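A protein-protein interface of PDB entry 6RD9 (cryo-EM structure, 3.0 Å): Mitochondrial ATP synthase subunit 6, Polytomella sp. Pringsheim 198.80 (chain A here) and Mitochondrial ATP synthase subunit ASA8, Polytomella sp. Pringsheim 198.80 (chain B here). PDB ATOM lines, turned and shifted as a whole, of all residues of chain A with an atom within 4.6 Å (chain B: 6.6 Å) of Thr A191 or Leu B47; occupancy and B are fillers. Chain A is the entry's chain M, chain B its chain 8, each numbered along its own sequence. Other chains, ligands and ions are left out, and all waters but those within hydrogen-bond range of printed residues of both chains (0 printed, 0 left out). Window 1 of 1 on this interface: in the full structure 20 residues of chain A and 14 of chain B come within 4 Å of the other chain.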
ATOM      1  N   TRP A 151      21.964 -11.242  24.816  1.00  0.00           N
ATOM      2  CA  TRP A 151      21.030 -10.404  24.082  1.00  0.00           C
ATOM      3  C   TRP A 151      20.010 -11.230  23.337  1.00  0.00           C
ATOM      4  O   TRP A 151      18.854 -10.843  23.255  1.00  0.00           O
ATOM      5  CB  TRP A 151      21.754  -9.527  23.087  1.00  0.00           C
ATOM      6  CG  TRP A 151      22.703  -8.605  23.654  1.00  0.00           C
ATOM      7  CD1 TRP A 151      22.790  -8.208  24.932  1.00  0.00           C
ATOM      8  CD2 TRP A 151      23.734  -7.941  22.953  1.00  0.00           C
ATOM      9  NE1 TRP A 151      23.813  -7.331  25.080  1.00  0.00           N
ATOM     10  CE2 TRP A 151      24.403  -7.141  23.866  1.00  0.00           C
ATOM     11  CE3 TRP A 151      24.143  -7.931  21.629  1.00  0.00           C
ATOM     12  CZ2 TRP A 151      25.466  -6.366  23.512  1.00  0.00           C
ATOM     13  CZ3 TRP A 151      25.190  -7.165  21.286  1.00  0.00           C
ATOM     14  CH2 TRP A 151      25.841  -6.389  22.211  1.00  0.00           C
ATOM     15  N   PHE A 155      15.912 -11.232  23.786  1.00  0.00           N
ATOM     16  CA  PHE A 155      14.926 -11.057  22.736  1.00  0.00           C
ATOM     17  C   PHE A 155      14.137 -12.318  22.479  1.00  0.00           C
ATOM     18  O   PHE A 155      13.057 -12.249  21.921  1.00  0.00           O
ATOM     19  CB  PHE A 155      15.609 -10.615  21.461  1.00  0.00           C
ATOM     20  CG  PHE A 155      16.052  -9.214  21.501  1.00  0.00           C
ATOM     21  CD1 PHE A 155      15.143  -8.210  21.680  1.00  0.00           C
ATOM     22  CD2 PHE A 155      17.370  -8.892  21.364  1.00  0.00           C
ATOM     23  CE1 PHE A 155      15.542  -6.922  21.720  1.00  0.00           C
ATOM     24  CE2 PHE A 155      17.773  -7.598  21.418  1.00  0.00           C
ATOM     25  CZ  PHE A 155      16.855  -6.614  21.592  1.00  0.00           C
ATOM     26  N   SER A 187      16.036  -1.879  17.046  1.00  0.00           N
ATOM     27  CA  SER A 187      16.953  -1.856  18.169  1.00  0.00           C
ATOM     28  C   SER A 187      17.981  -2.964  18.098  1.00  0.00           C
ATOM     29  O   SER A 187      19.063  -2.833  18.663  1.00  0.00           O
ATOM     30  CB  SER A 187      16.160  -1.972  19.437  1.00  0.00           C
ATOM     31  OG  SER A 187      15.316  -0.860  19.550  1.00  0.00           O
ATOM     32  N   VAL A 188      17.643  -4.080  17.468  1.00  0.00           N
ATOM     33  CA  VAL A 188      18.637  -5.088  17.146  1.00  0.00           C
ATOM     34  C   VAL A 188      19.540  -4.605  16.034  1.00  0.00           C
ATOM     35  O   VAL A 188      20.755  -4.815  16.067  1.00  0.00           O
ATOM     36  CB  VAL A 188      17.934  -6.390  16.766  1.00  0.00           C
ATOM     37  CG1 VAL A 188      18.912  -7.403  16.384  1.00  0.00           C
ATOM     38  CG2 VAL A 188      17.220  -6.875  17.923  1.00  0.00           C
ATOM     39  N   TRP A 189      18.970  -3.957  15.031  1.00  0.00           N
ATOM     40  CA  TRP A 189      19.768  -3.477  13.919  1.00  0.00           C
ATOM     41  C   TRP A 189      20.688  -2.353  14.346  1.00  0.00           C
ATOM     42  O   TRP A 189      21.785  -2.209  13.812  1.00  0.00           O
ATOM     43  CB  TRP A 189      18.854  -3.025  12.797  1.00  0.00           C
ATOM     44  CG  TRP A 189      19.556  -2.363  11.678  1.00  0.00           C
ATOM     45  CD1 TRP A 189      20.069  -2.957  10.585  1.00  0.00           C
ATOM     46  CD2 TRP A 189      19.811  -0.971  11.535  1.00  0.00           C
ATOM     47  NE1 TRP A 189      20.639  -2.032   9.772  1.00  0.00           N
ATOM     48  CE2 TRP A 189      20.495  -0.799  10.340  1.00  0.00           C
ATOM     49  CE3 TRP A 189      19.540   0.144  12.317  1.00  0.00           C
ATOM     50  CZ2 TRP A 189      20.904   0.431   9.908  1.00  0.00           C
ATOM     51  CZ3 TRP A 189      19.952   1.352  11.890  1.00  0.00           C
ATOM     52  CH2 TRP A 189      20.620   1.494  10.700  1.00  0.00           C
ATOM     53  N   ALA A 190      20.255  -1.525  15.281  1.00  0.00           N
ATOM     54  CA  ALA A 190      21.127  -0.466  15.736  1.00  0.00           C
ATOM     55  C   ALA A 190      22.193  -0.995  16.665  1.00  0.00           C
ATOM     56  O   ALA A 190      23.288  -0.449  16.706  1.00  0.00           O
ATOM     57  CB  ALA A 190      20.316   0.616  16.416  1.00  0.00           C
ATOM     58  N   THR A 191      21.900  -2.055  17.405  1.00  0.00           N
ATOM     59  CA  THR A 191      22.889  -2.691  18.260  1.00  0.00           C
ATOM     60  C   THR A 191      23.977  -3.347  17.440  1.00  0.00           C
ATOM     61  O   THR A 191      25.146  -3.324  17.823  1.00  0.00           O
ATOM     62  CB  THR A 191      22.193  -3.719  19.121  1.00  0.00           C
ATOM     63  OG1 THR A 191      21.087  -3.095  19.761  1.00  0.00           O
ATOM     64  CG2 THR A 191      23.094  -4.276  20.140  1.00  0.00           C
ATOM     65  N   ALA A 192      23.610  -3.939  16.311  1.00  0.00           N
ATOM     66  CA  ALA A 192      24.606  -4.488  15.416  1.00  0.00           C
ATOM     67  C   ALA A 192      25.449  -3.391  14.804  1.00  0.00           C
ATOM     68  O   ALA A 192      26.661  -3.538  14.695  1.00  0.00           O
ATOM     69  CB  ALA A 192      23.927  -5.298  14.329  1.00  0.00           C
ATOM     70  N   THR A 193      24.837  -2.268  14.458  1.00  0.00           N
ATOM     71  CA  THR A 193      25.562  -1.184  13.817  1.00  0.00           C
ATOM     72  C   THR A 193      26.456  -0.443  14.798  1.00  0.00           C
ATOM     73  O   THR A 193      27.593  -0.116  14.463  1.00  0.00           O
ATOM     74  CB  THR A 193      24.563  -0.258  13.157  1.00  0.00           C
ATOM     75  OG1 THR A 193      23.763  -1.037  12.274  1.00  0.00           O
ATOM     76  CG2 THR A 193      25.247   0.786  12.356  1.00  0.00           C
ATOM     77  N   ILE A 194      25.979  -0.196  16.018  1.00  0.00           N
ATOM     78  CA  ILE A 194      26.799   0.431  17.050  1.00  0.00           C
ATOM     79  C   ILE A 194      27.967  -0.463  17.422  1.00  0.00           C
ATOM     80  O   ILE A 194      29.072   0.020  17.677  1.00  0.00           O
ATOM     81  CB  ILE A 194      25.915   0.775  18.258  1.00  0.00           C
ATOM     82  CG1 ILE A 194      25.045   1.959  17.926  1.00  0.00           C
ATOM     83  CG2 ILE A 194      26.704   1.187  19.428  1.00  0.00           C
ATOM     84  CD1 ILE A 194      24.050   2.245  18.939  1.00  0.00           C
ATOM     85  N   LEU A 195      27.771  -1.775  17.400  1.00  0.00           N
ATOM     86  CA  LEU A 195      28.884  -2.691  17.589  1.00  0.00           C
ATOM     87  C   LEU A 195      29.855  -2.629  16.423  1.00  0.00           C
ATOM     88  O   LEU A 195      31.066  -2.602  16.626  1.00  0.00           O
ATOM     89  CB  LEU A 195      28.356  -4.105  17.773  1.00  0.00           C
ATOM     90  CG  LEU A 195      29.343  -5.242  17.915  1.00  0.00           C
ATOM     91  CD1 LEU A 195      29.824  -5.332  19.295  1.00  0.00           C
ATOM     92  CD2 LEU A 195      28.644  -6.477  17.574  1.00  0.00           C
ATOM     93  N   ARG B  43      29.333  -4.021  28.993  1.00  0.00           N
ATOM     94  CA  ARG B  43      28.975  -5.111  28.108  1.00  0.00           C
ATOM     95  C   ARG B  43      27.740  -4.861  27.280  1.00  0.00           C
ATOM     96  O   ARG B  43      27.689  -5.322  26.148  1.00  0.00           O
ATOM     97  CB  ARG B  43      28.756  -6.401  28.897  1.00  0.00           C
ATOM     98  CG  ARG B  43      29.914  -6.841  29.681  1.00  0.00           C
ATOM     99  CD  ARG B  43      30.992  -7.309  28.764  1.00  0.00           C
ATOM    100  NE  ARG B  43      30.717  -8.620  28.217  1.00  0.00           N
ATOM    101  CZ  ARG B  43      31.253  -9.070  27.101  1.00  0.00           C
ATOM    102  NH1 ARG B  43      32.069  -8.301  26.428  1.00  0.00           N
ATOM    103  NH2 ARG B  43      30.974 -10.277  26.661  1.00  0.00           N
ATOM    104  N   HIS B  44      26.735  -4.182  27.819  1.00  0.00           N
ATOM    105  CA  HIS B  44      25.466  -4.023  27.136  1.00  0.00           C
ATOM    106  C   HIS B  44      25.203  -2.598  26.709  1.00  0.00           C
ATOM    107  O   HIS B  44      24.048  -2.234  26.553  1.00  0.00           O
ATOM    108  CB  HIS B  44      24.299  -4.467  28.011  1.00  0.00           C
ATOM    109  CG  HIS B  44      24.456  -5.819  28.622  1.00  0.00           C
ATOM    110  ND1 HIS B  44      24.850  -6.922  27.910  1.00  0.00           N
ATOM    111  CD2 HIS B  44      24.233  -6.245  29.879  1.00  0.00           C
ATOM    112  CE1 HIS B  44      24.899  -7.965  28.711  1.00  0.00           C
ATOM    113  NE2 HIS B  44      24.525  -7.580  29.912  1.00  0.00           N
ATOM    114  N   TRP B  45      26.221  -1.770  26.536  1.00  0.00           N
ATOM    115  CA  TRP B  45      25.940  -0.420  26.072  1.00  0.00           C
ATOM    116  C   TRP B  45      25.596  -0.374  24.598  1.00  0.00           C
ATOM    117  O   TRP B  45      25.076   0.637  24.133  1.00  0.00           O
ATOM    118  CB  TRP B  45      27.112   0.511  26.353  1.00  0.00           C
ATOM    119  CG  TRP B  45      28.291   0.319  25.494  1.00  0.00           C
ATOM    120  CD1 TRP B  45      29.327  -0.502  25.721  1.00  0.00           C
ATOM    121  CD2 TRP B  45      28.573   0.991  24.270  1.00  0.00           C
ATOM    122  NE1 TRP B  45      30.238  -0.406  24.715  1.00  0.00           N
ATOM    123  CE2 TRP B  45      29.784   0.501  23.802  1.00  0.00           C
ATOM    124  CE3 TRP B  45      27.899   1.943  23.513  1.00  0.00           C
ATOM    125  CZ2 TRP B  45      30.343   0.936  22.626  1.00  0.00           C
ATOM    126  CZ3 TRP B  45      28.449   2.359  22.358  1.00  0.00           C
ATOM    127  CH2 TRP B  45      29.655   1.862  21.920  1.00  0.00           C
ATOM    128  N   TYR B  46      25.878  -1.436  23.856  1.00  0.00           N
ATOM    129  CA  TYR B  46      25.421  -1.524  22.485  1.00  0.00           C
ATOM    130  C   TYR B  46      23.916  -1.692  22.421  1.00  0.00           C
ATOM    131  O   TYR B  46      23.277  -1.146  21.527  1.00  0.00           O
ATOM    132  CB  TYR B  46      26.095  -2.687  21.788  1.00  0.00           C
ATOM    133  CG  TYR B  46      27.556  -2.816  22.045  1.00  0.00           C
ATOM    134  CD1 TYR B  46      28.466  -2.149  21.269  1.00  0.00           C
ATOM    135  CD2 TYR B  46      28.027  -3.636  23.039  1.00  0.00           C
ATOM    136  CE1 TYR B  46      29.793  -2.282  21.486  1.00  0.00           C
ATOM    137  CE2 TYR B  46      29.345  -3.764  23.269  1.00  0.00           C
ATOM    138  CZ  TYR B  46      30.224  -3.086  22.493  1.00  0.00           C
ATOM    139  OH  TYR B  46      31.562  -3.226  22.733  1.00  0.00           O
ATOM    140  N   LEU B  47      23.328  -2.455  23.342  1.00  0.00           N
ATOM    141  CA  LEU B  47      21.874  -2.558  23.378  1.00  0.00           C
ATOM    142  C   LEU B  47      21.233  -1.277  23.846  1.00  0.00           C
ATOM    143  O   LEU B  47      20.197  -0.878  23.320  1.00  0.00           O
ATOM    144  CB  LEU B  47      21.401  -3.663  24.297  1.00  0.00           C
ATOM    145  CG  LEU B  47      21.043  -5.015  23.761  1.00  0.00           C
ATOM    146  CD1 LEU B  47      20.293  -5.690  24.841  1.00  0.00           C
ATOM    147  CD2 LEU B  47      20.175  -4.860  22.565  1.00  0.00           C
ATOM    148  N   LEU B  48      21.793  -0.651  24.869  1.00  0.00           N
ATOM    149  CA  LEU B  48      21.214   0.579  25.372  1.00  0.00           C
ATOM    150  C   LEU B  48      21.382   1.709  24.383  1.00  0.00           C
ATOM    151  O   LEU B  48      20.587   2.642  24.375  1.00  0.00           O
ATOM    152  CB  LEU B  48      21.854   0.957  26.692  1.00  0.00           C
ATOM    153  CG  LEU B  48      21.826  -0.045  27.826  1.00  0.00           C
ATOM    154  CD1 LEU B  48      22.330   0.668  29.037  1.00  0.00           C
ATOM    155  CD2 LEU B  48      20.449  -0.584  28.044  1.00  0.00           C
ATOM    156  N   GLY B  49      22.416   1.653  23.554  1.00  0.00           N
ATOM    157  CA  GLY B  49      22.507   2.579  22.452  1.00  0.00           C
ATOM    158  C   GLY B  49      21.531   2.263  21.353  1.00  0.00           C
ATOM    159  O   GLY B  49      21.063   3.167  20.668  1.00  0.00           O
ATOM    160  N   GLY B  50      21.212   0.992  21.156  1.00  0.00           N
ATOM    161  CA  GLY B  50      20.248   0.632  20.141  1.00  0.00           C
ATOM    162  C   GLY B  50      18.821   0.902  20.553  1.00  0.00           C
ATOM    163  O   GLY B  50      17.977   1.178  19.707  1.00  0.00           O
ATOM    164  N   PHE B  51      18.519   0.791  21.843  1.00  0.00           N
ATOM    165  CA  PHE B  51      17.213   1.207  22.326  1.00  0.00           C
ATOM    166  C   PHE B  51      17.090   2.717  22.336  1.00  0.00           C
ATOM    167  O   PHE B  51      15.991   3.243  22.209  1.00  0.00           O
ATOM    168  CB  PHE B  51      16.962   0.672  23.732  1.00  0.00           C
ATOM    169  CG  PHE B  51      16.708  -0.795  23.793  1.00  0.00           C
ATOM    170  CD1 PHE B  51      15.895  -1.403  22.876  1.00  0.00           C
ATOM    171  CD2 PHE B  51      17.259  -1.558  24.791  1.00  0.00           C
ATOM    172  CE1 PHE B  51      15.659  -2.744  22.922  1.00  0.00           C
ATOM    173  CE2 PHE B  51      17.015  -2.897  24.850  1.00  0.00           C
ATOM    174  CZ  PHE B  51      16.219  -3.487  23.906  1.00  0.00           C
ATOM    175  N   THR B  52      18.199   3.429  22.505  1.00  0.00           N
ATOM    176  CA  THR B  52      18.170   4.886  22.474  1.00  0.00           C
ATOM    177  C   THR B  52      17.988   5.394  21.059  1.00  0.00           C
ATOM    178  O   THR B  52      17.305   6.396  20.840  1.00  0.00           O
ATOM    179  CB  THR B  52      19.452   5.436  23.085  1.00  0.00           C
ATOM    180  OG1 THR B  52      19.552   4.974  24.429  1.00  0.00           O
ATOM    181  CG2 THR B  52      19.462   6.930  23.125  1.00  0.00           C
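Among the printed residues, pairs that only touch across the chains: Trp A151 with Arg B43 (3.6 Å), Trp A151 with Tyr B46 (3.6 Å), Trp A151 with Leu B47 (3.5 Å), Phe A155 with Leu B47 (3.8 Å), Phe A155 with Phe B51 (3.9 Å), Ser A187 with Phe B51 (3.4 Å), Ala A190 with Gly B50 (3.7 Å), Thr A191 with Leu B47 (3.4 Å), Thr A191 with Gly B50 (3.8 Å), Ile A194 with Trp B45 (3.6 Å), Ile A194 with Gly B49 (3.5 Å), Ile A194 with Gly B50 (3.8 Å) and Leu A195 with Tyr B46 (3.7 Å).
Of chain B, only Tyr B46 (3.4 Å), Leu B47 (3.4 Å) and Gly B50 (3.8 Å) come within 4 Å of Thr A191.
Leu B47 touches just these residues of chain A: Trp A151 (3.5 Å), Phe A155 (3.8 Å) and Thr A191 (3.4 Å).
Printed residues of chain B within 4 Å of Phe A155: Leu B47 and Phe B51.
Of the printed residues of chain A, Gly B49 touches Ile A194 (3.5 Å).
Of the printed residues of chain B, Leu A195 touches Tyr B46 (3.7 Å).
The nearest residue of chain A that does not touch Leu B47 is Ser A187 (4.5 Å).
The nearest printed residue of chain B that does not touch Ala A190 is Tyr B46 (4.9 Å).
OG of Ser A187 sits at hydrogen-bond distance from O of Gly B50 (3.4 Å).
NE1 of Trp A151 sits at hydrogen-bond distance from ND1 of His B44, at 3.0 Å.
The side-chain hydroxyl (OG1) of Thr A191 lies within hydrogen-bond range of the backbone carbonyl oxygen (O) of Tyr B46.
Of the 11 printed residues of chain A, 7 touch a printed residue of chain B.
Hydrophobic or aromatic side chains of chain A that line the printed part of chain B: Trp A151, Phe A155, Ala A190, Ile A194 and Leu A195.
Along chain A the printed residues that touch a printed residue of chain B span positions 151 to 195.
Hydrophobic or aromatic side chains of chain B within 4 Å of the printed part of chain A: His B44, Trp B45, Tyr B46, Leu B47 and Phe B51.
Along chain B the printed residues that touch a printed residue of chain A span positions 43 to 51.
Among the printed residues, no Asp or Glu carboxylate lies within 4 Å of a Lys or Arg side-chain nitrogen of the other chain.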
